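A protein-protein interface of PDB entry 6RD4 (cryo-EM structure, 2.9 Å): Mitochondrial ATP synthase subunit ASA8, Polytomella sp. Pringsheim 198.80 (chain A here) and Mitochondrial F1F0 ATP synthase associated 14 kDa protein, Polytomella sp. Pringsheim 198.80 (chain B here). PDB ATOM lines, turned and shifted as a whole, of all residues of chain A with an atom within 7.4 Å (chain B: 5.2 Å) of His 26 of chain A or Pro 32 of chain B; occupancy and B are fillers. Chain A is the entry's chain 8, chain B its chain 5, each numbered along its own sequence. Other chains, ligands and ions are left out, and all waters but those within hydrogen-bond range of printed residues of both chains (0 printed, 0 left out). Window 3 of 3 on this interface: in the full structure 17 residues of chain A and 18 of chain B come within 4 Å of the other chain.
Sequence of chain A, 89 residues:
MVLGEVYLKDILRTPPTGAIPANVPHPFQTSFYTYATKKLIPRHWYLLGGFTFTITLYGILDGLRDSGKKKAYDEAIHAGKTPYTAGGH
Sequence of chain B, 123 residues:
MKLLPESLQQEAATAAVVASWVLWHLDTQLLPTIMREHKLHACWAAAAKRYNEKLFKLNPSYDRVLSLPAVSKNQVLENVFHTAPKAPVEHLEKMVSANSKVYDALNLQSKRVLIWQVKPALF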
ATOM      1  N   ASN A  23       9.694 -38.342 -16.646  1.00  0.00           N
ATOM      2  CA  ASN A  23       9.085 -37.993 -15.376  1.00  0.00           C
ATOM      3  C   ASN A  23       7.677 -37.485 -15.615  1.00  0.00           C
ATOM      4  O   ASN A  23       7.397 -36.847 -16.628  1.00  0.00           O
ATOM      5  CB  ASN A  23       9.928 -36.946 -14.674  1.00  0.00           C
ATOM      6  CG  ASN A  23       9.611 -36.827 -13.225  1.00  0.00           C
ATOM      7  OD1 ASN A  23       8.744 -37.510 -12.716  1.00  0.00           O
ATOM      8  ND2 ASN A  23      10.333 -35.970 -12.539  1.00  0.00           N
ATOM      9  N   VAL A  24       6.778 -37.823 -14.709  1.00  0.00           N
ATOM     10  CA  VAL A  24       5.397 -37.357 -14.802  1.00  0.00           C
ATOM     11  C   VAL A  24       5.345 -35.908 -14.332  1.00  0.00           C
ATOM     12  O   VAL A  24       5.799 -35.614 -13.221  1.00  0.00           O
ATOM     13  CB  VAL A  24       4.486 -38.237 -13.970  1.00  0.00           C
ATOM     14  CG1 VAL A  24       3.135 -37.653 -13.892  1.00  0.00           C
ATOM     15  CG2 VAL A  24       4.398 -39.553 -14.580  1.00  0.00           C
ATOM     16  N   PRO A  25       4.829 -34.987 -15.129  1.00  0.00           N
ATOM     17  CA  PRO A  25       4.749 -33.605 -14.690  1.00  0.00           C
ATOM     18  C   PRO A  25       3.667 -33.418 -13.654  1.00  0.00           C
ATOM     19  O   PRO A  25       2.630 -34.076 -13.673  1.00  0.00           O
ATOM     20  CB  PRO A  25       4.390 -32.858 -15.972  1.00  0.00           C
ATOM     21  CG  PRO A  25       4.614 -33.788 -17.027  1.00  0.00           C
ATOM     22  CD  PRO A  25       4.343 -35.118 -16.495  1.00  0.00           C
ATOM     23  N   HIS A  26       3.926 -32.513 -12.741  1.00  0.00           N
ATOM     24  CA  HIS A  26       2.858 -32.008 -11.928  1.00  0.00           C
ATOM     25  C   HIS A  26       1.936 -31.165 -12.802  1.00  0.00           C
ATOM     26  O   HIS A  26       2.361 -30.649 -13.831  1.00  0.00           O
ATOM     27  CB  HIS A  26       3.422 -31.181 -10.791  1.00  0.00           C
ATOM     28  CG  HIS A  26       2.418 -30.853  -9.752  1.00  0.00           C
ATOM     29  ND1 HIS A  26       2.080 -31.719  -8.751  1.00  0.00           N
ATOM     30  CD2 HIS A  26       1.620 -29.783  -9.603  1.00  0.00           C
ATOM     31  CE1 HIS A  26       1.139 -31.177  -8.008  1.00  0.00           C
ATOM     32  NE2 HIS A  26       0.839 -30.002  -8.509  1.00  0.00           N
ATOM     33  N   PRO A  27       0.658 -31.044 -12.443  1.00  0.00           N
ATOM     34  CA  PRO A  27      -0.225 -30.125 -13.167  1.00  0.00           C
ATOM     35  C   PRO A  27       0.207 -28.673 -13.170  1.00  0.00           C
ATOM     36  O   PRO A  27      -0.235 -27.928 -14.039  1.00  0.00           O
ATOM     37  CB  PRO A  27      -1.543 -30.302 -12.433  1.00  0.00           C
ATOM     38  CG  PRO A  27      -1.522 -31.689 -12.069  1.00  0.00           C
ATOM     39  CD  PRO A  27      -0.133 -32.062 -11.746  1.00  0.00           C
ATOM     40  N   PHE A  28       1.050 -28.249 -12.241  1.00  0.00           N
ATOM     41  CA  PHE A  28       1.557 -26.893 -12.187  1.00  0.00           C
ATOM     42  C   PHE A  28       2.744 -26.707 -13.103  1.00  0.00           C
ATOM     43  O   PHE A  28       2.974 -25.607 -13.595  1.00  0.00           O
ATOM     44  CB  PHE A  28       1.987 -26.548 -10.773  1.00  0.00           C
ATOM     45  CG  PHE A  28       0.875 -26.431  -9.794  1.00  0.00           C
ATOM     46  CD1 PHE A  28      -0.430 -26.329 -10.190  1.00  0.00           C
ATOM     47  CD2 PHE A  28       1.153 -26.366  -8.461  1.00  0.00           C
ATOM     48  CE1 PHE A  28      -1.412 -26.204  -9.283  1.00  0.00           C
ATOM     49  CE2 PHE A  28       0.167 -26.235  -7.567  1.00  0.00           C
ATOM     50  CZ  PHE A  28      -1.109 -26.143  -7.983  1.00  0.00           C
ATOM     51  N   GLN A  29       3.532 -27.750 -13.308  1.00  0.00           N
ATOM     52  CA  GLN A  29       4.624 -27.662 -14.256  1.00  0.00           C
ATOM     53  C   GLN A  29       4.123 -27.713 -15.675  1.00  0.00           C
ATOM     54  O   GLN A  29       4.794 -27.235 -16.588  1.00  0.00           O
ATOM     55  CB  GLN A  29       5.606 -28.791 -14.043  1.00  0.00           C
ATOM     56  CG  GLN A  29       5.989 -28.988 -12.647  1.00  0.00           C
ATOM     57  CD  GLN A  29       7.061 -29.976 -12.541  1.00  0.00           C
ATOM     58  OE1 GLN A  29       7.864 -30.100 -13.434  1.00  0.00           O
ATOM     59  NE2 GLN A  29       7.114 -30.677 -11.441  1.00  0.00           N
ATOM     60  N   THR A  30       2.962 -28.312 -15.881  1.00  0.00           N
ATOM     61  CA  THR A  30       2.380 -28.372 -17.211  1.00  0.00           C
ATOM     62  C   THR A  30       1.925 -26.998 -17.669  1.00  0.00           C
ATOM     63  O   THR A  30       2.354 -26.515 -18.714  1.00  0.00           O
ATOM     64  CB  THR A  30       1.221 -29.357 -17.220  1.00  0.00           C
ATOM     65  OG1 THR A  30       1.738 -30.681 -17.106  1.00  0.00           O
ATOM     66  CG2 THR A  30       0.430 -29.246 -18.479  1.00  0.00           C
ATOM     67  N   SER A  31       1.090 -26.338 -16.887  1.00  0.00           N
ATOM     68  CA  SER A  31       0.487 -25.091 -17.312  1.00  0.00           C
ATOM     69  C   SER A  31       0.533 -24.053 -16.215  1.00  0.00           C
ATOM     70  O   SER A  31       0.237 -24.350 -15.062  1.00  0.00           O
ATOM     71  CB  SER A  31      -0.943 -25.308 -17.717  1.00  0.00           C
ATOM     72  OG  SER A  31      -1.666 -25.825 -16.636  1.00  0.00           O
ATOM     73  N   THR A  34      -3.032 -23.432 -14.649  1.00  0.00           N
ATOM     74  CA  THR A  34      -3.470 -24.247 -13.526  1.00  0.00           C
ATOM     75  C   THR A  34      -2.826 -23.781 -12.241  1.00  0.00           C
ATOM     76  O   THR A  34      -3.453 -23.831 -11.188  1.00  0.00           O
ATOM     77  CB  THR A  34      -3.121 -25.704 -13.757  1.00  0.00           C
ATOM     78  OG1 THR A  34      -3.429 -26.039 -15.108  1.00  0.00           O
ATOM     79  CG2 THR A  34      -3.923 -26.585 -12.866  1.00  0.00           C
ATOM     80  N   LYS A  39      -3.566 -22.124  -7.428  1.00  0.00           N
ATOM     81  CA  LYS A  39      -2.723 -21.873  -6.279  1.00  0.00           C
ATOM     82  C   LYS A  39      -2.282 -20.437  -6.144  1.00  0.00           C
ATOM     83  O   LYS A  39      -2.313 -19.913  -5.046  1.00  0.00           O
ATOM     84  CB  LYS A  39      -1.509 -22.750  -6.321  1.00  0.00           C
ATOM     85  CG  LYS A  39      -0.629 -22.599  -5.143  1.00  0.00           C
ATOM     86  CD  LYS A  39       0.267 -23.728  -5.037  1.00  0.00           C
ATOM     87  CE  LYS A  39      -0.319 -24.765  -4.200  1.00  0.00           C
ATOM     88  NZ  LYS A  39      -0.302 -24.296  -2.830  1.00  0.00           N
ATOM     89  N   LEU B  26       9.326 -22.202  -6.526  1.00  0.00           N
ATOM     90  CA  LEU B  26       9.155 -23.074  -5.386  1.00  0.00           C
ATOM     91  C   LEU B  26       7.851 -23.840  -5.476  1.00  0.00           C
ATOM     92  O   LEU B  26       7.833 -25.052  -5.312  1.00  0.00           O
ATOM     93  CB  LEU B  26       9.199 -22.245  -4.128  1.00  0.00           C
ATOM     94  CG  LEU B  26       9.171 -22.879  -2.782  1.00  0.00           C
ATOM     95  CD1 LEU B  26      10.526 -23.372  -2.491  1.00  0.00           C
ATOM     96  CD2 LEU B  26       8.792 -21.781  -1.894  1.00  0.00           C
ATOM     97  N   ASP B  27       6.751 -23.153  -5.763  1.00  0.00           N
ATOM     98  CA  ASP B  27       5.440 -23.781  -5.758  1.00  0.00           C
ATOM     99  C   ASP B  27       5.244 -24.759  -6.881  1.00  0.00           C
ATOM    100  O   ASP B  27       4.441 -25.679  -6.760  1.00  0.00           O
ATOM    101  CB  ASP B  27       4.363 -22.751  -5.916  1.00  0.00           C
ATOM    102  CG  ASP B  27       3.822 -22.280  -4.644  1.00  0.00           C
ATOM    103  OD1 ASP B  27       3.854 -23.026  -3.659  1.00  0.00           O
ATOM    104  OD2 ASP B  27       3.282 -21.172  -4.647  1.00  0.00           O
ATOM    105  N   THR B  28       5.903 -24.540  -7.995  1.00  0.00           N
ATOM    106  CA  THR B  28       5.669 -25.292  -9.207  1.00  0.00           C
ATOM    107  C   THR B  28       6.744 -26.332  -9.447  1.00  0.00           C
ATOM    108  O   THR B  28       6.440 -27.469  -9.768  1.00  0.00           O
ATOM    109  CB  THR B  28       5.572 -24.314 -10.364  1.00  0.00           C
ATOM    110  OG1 THR B  28       4.324 -23.644 -10.309  1.00  0.00           O
ATOM    111  CG2 THR B  28       5.700 -24.956 -11.648  1.00  0.00           C
ATOM    112  N   GLN B  29       8.002 -25.980  -9.252  1.00  0.00           N
ATOM    113  CA  GLN B  29       9.095 -26.874  -9.571  1.00  0.00           C
ATOM    114  C   GLN B  29       9.714 -27.527  -8.355  1.00  0.00           C
ATOM    115  O   GLN B  29       9.943 -28.730  -8.368  1.00  0.00           O
ATOM    116  CB  GLN B  29      10.162 -26.127 -10.356  1.00  0.00           C
ATOM    117  CG  GLN B  29       9.601 -25.261 -11.438  1.00  0.00           C
ATOM    118  CD  GLN B  29       9.207 -26.039 -12.635  1.00  0.00           C
ATOM    119  OE1 GLN B  29       8.360 -25.628 -13.412  1.00  0.00           O
ATOM    120  NE2 GLN B  29       9.827 -27.188 -12.815  1.00  0.00           N
ATOM    121  N   LEU B  30       9.994 -26.772  -7.307  1.00  0.00           N
ATOM    122  CA  LEU B  30      10.658 -27.371  -6.159  1.00  0.00           C
ATOM    123  C   LEU B  30       9.699 -28.160  -5.293  1.00  0.00           C
ATOM    124  O   LEU B  30       9.930 -29.336  -5.045  1.00  0.00           O
ATOM    125  CB  LEU B  30      11.356 -26.307  -5.337  1.00  0.00           C
ATOM    126  CG  LEU B  30      12.490 -25.605  -6.039  1.00  0.00           C
ATOM    127  CD1 LEU B  30      13.161 -24.733  -5.060  1.00  0.00           C
ATOM    128  CD2 LEU B  30      13.453 -26.582  -6.600  1.00  0.00           C
ATOM    129  N   LEU B  31       8.611 -27.548  -4.836  1.00  0.00           N
ATOM    130  CA  LEU B  31       7.751 -28.219  -3.868  1.00  0.00           C
ATOM    131  C   LEU B  31       6.963 -29.415  -4.382  1.00  0.00           C
ATOM    132  O   LEU B  31       6.591 -30.246  -3.544  1.00  0.00           O
ATOM    133  CB  LEU B  31       6.757 -27.243  -3.245  1.00  0.00           C
ATOM    134  CG  LEU B  31       7.089 -26.463  -1.995  1.00  0.00           C
ATOM    135  CD1 LEU B  31       5.869 -25.701  -1.624  1.00  0.00           C
ATOM    136  CD2 LEU B  31       7.468 -27.416  -0.927  1.00  0.00           C
ATOM    137  N   PRO B  32       6.612 -29.547  -5.659  1.00  0.00           N
ATOM    138  CA  PRO B  32       6.161 -30.851  -6.125  1.00  0.00           C
ATOM    139  C   PRO B  32       7.195 -31.939  -6.031  1.00  0.00           C
ATOM    140  O   PRO B  32       6.847 -33.065  -5.697  1.00  0.00           O
ATOM    141  CB  PRO B  32       5.769 -30.547  -7.560  1.00  0.00           C
ATOM    142  CG  PRO B  32       5.184 -29.293  -7.433  1.00  0.00           C
ATOM    143  CD  PRO B  32       6.030 -28.526  -6.536  1.00  0.00           C
ATOM    144  N   THR B  33       8.451 -31.644  -6.298  1.00  0.00           N
ATOM    145  CA  THR B  33       9.529 -32.604  -6.159  1.00  0.00           C
ATOM    146  C   THR B  33       9.851 -32.913  -4.706  1.00  0.00           C
ATOM    147  O   THR B  33      10.171 -34.058  -4.384  1.00  0.00           O
ATOM    148  CB  THR B  33      10.747 -32.041  -6.863  1.00  0.00           C
ATOM    149  OG1 THR B  33      10.403 -31.764  -8.219  1.00  0.00           O
ATOM    150  CG2 THR B  33      11.868 -32.980  -6.829  1.00  0.00           C
ATOM    151  N   ILE B  34       9.789 -31.908  -3.830  1.00  0.00           N
ATOM    152  CA  ILE B  34       9.994 -32.116  -2.400  1.00  0.00           C
ATOM    153  C   ILE B  34       8.971 -33.091  -1.872  1.00  0.00           C
ATOM    154  O   ILE B  34       9.308 -34.071  -1.218  1.00  0.00           O
ATOM    155  CB  ILE B  34       9.896 -30.787  -1.632  1.00  0.00           C
ATOM    156  CG1 ILE B  34      10.969 -29.790  -2.022  1.00  0.00           C
ATOM    157  CG2 ILE B  34       9.918 -31.010  -0.162  1.00  0.00           C
ATOM    158  CD1 ILE B  34      12.273 -30.270  -1.929  1.00  0.00           C
ATOM    159  N   MET B  35       7.709 -32.852  -2.177  1.00  0.00           N
ATOM    160  CA  MET B  35       6.625 -33.623  -1.612  1.00  0.00           C
ATOM    161  C   MET B  35       6.438 -34.954  -2.291  1.00  0.00           C
ATOM    162  O   MET B  35       5.761 -35.806  -1.743  1.00  0.00           O
ATOM    163  CB  MET B  35       5.330 -32.839  -1.690  1.00  0.00           C
ATOM    164  CG  MET B  35       5.281 -31.662  -0.805  1.00  0.00           C
ATOM    165  SD  MET B  35       5.935 -32.014   0.802  1.00  0.00           S
ATOM    166  CE  MET B  35       6.365 -30.379   1.278  1.00  0.00           C
ATOM    167  N   ARG B  36       7.009 -35.170  -3.457  1.00  0.00           N
ATOM    168  CA  ARG B  36       6.889 -36.478  -4.062  1.00  0.00           C
ATOM    169  C   ARG B  36       7.798 -37.461  -3.381  1.00  0.00           C
ATOM    170  O   ARG B  36       7.499 -38.649  -3.326  1.00  0.00           O
ATOM    171  CB  ARG B  36       7.213 -36.408  -5.536  1.00  0.00           C
ATOM    172  CG  ARG B  36       6.036 -36.200  -6.380  1.00  0.00           C
ATOM    173  CD  ARG B  36       6.477 -36.016  -7.761  1.00  0.00           C
ATOM    174  NE  ARG B  36       5.395 -35.579  -8.607  1.00  0.00           N
ATOM    175  CZ  ARG B  36       5.348 -35.836  -9.896  1.00  0.00           C
ATOM    176  NH1 ARG B  36       4.331 -35.427 -10.617  1.00  0.00           N
ATOM    177  NH2 ARG B  36       6.321 -36.529 -10.445  1.00  0.00           N
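OD1 of Asn 23 of chain A sits at hydrogen-bond distance from NH2 of Arg 36 of chain B, at 3.5 Å.
NH2 of Arg 36 of chain B sits at hydrogen-bond distance from O of Val 24 of chain A (3.0 Å).
Pro 25 of chain A touches Arg 36 of chain B.
CG of Pro 32 of chain B touches CG of His 26 of chain A, at 3.9 Å.
His 26 of chain A touches Arg 36 of chain B.
Asp 27 of chain B touches Phe 28 of chain A (O to CD2, 3.8 Å).
Thr 28 of chain B touches Phe 28 of chain A.
Thr 28 of chain B touches Gln 29 of chain A.
OE1 of Gln 29 of chain A touches NE2 of Gln 29 of chain B (3.6 Å).
CD of Lys 39 of chain A touches CG of Asp 27 of chain B (3.9 Å).
Printed residues of chain A that touch a printed residue of chain B: Asn 23, Val 24, Pro 25, His 26, Phe 28, Gln 29 and Lys 39.
Hydrophobic or aromatic side chains of chain A that line the printed part of chain B: His 26 and Phe 28.
Of the 11 printed residues of chain B, 5 touch a printed residue of chain A.
Along chain B the printed residues that touch a printed residue of chain A span positions 27 to 36.
Among the printed residues, 10 pairs touch across the chains.
Among the printed residues, no Asp or Glu carboxylate lies within 4 Å of a Lys or Arg side-chain nitrogen of the other chain.
His 26 of chain A touches just these residues of chain B: Pro 32 and Arg 36.
Pro 32 of chain B touches just one residue of chain A: His 26.
Of the printed residues of chain A, Arg 36 of chain B touches Asn 23 (3.5 Å), Val 24 (3.0 Å), Pro 25 (3.7 Å) and His 26 (3.6 Å).
Of the printed residues of chain A, Gln 29 of chain B touches Gln 29 (3.6 Å).
Of the printed residues of chain A, Thr 28 of chain B touches Phe 28 (3.4 Å) and Gln 29 (3.3 Å).
Of the printed residues of chain B, Lys 39 of chain A touches Asp 27.
Of the printed residues of chain B, Gln 29 of chain A touches Thr 28 (3.3 Å) and Gln 29 (3.6 Å).
The nearest residue of chain B that does not touch His 26 of chain A is Thr 28 of chain B (4.9 Å).
The backbone carbonyl oxygen of Gln 29 of chain B sits at hydrogen-bond distance from the side-chain hydroxyl of Thr 33 of chain B.
OG1 of Thr 30 of chain A is in hydrogen-bond range of O of His 26 of chain A (3.3 Å).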
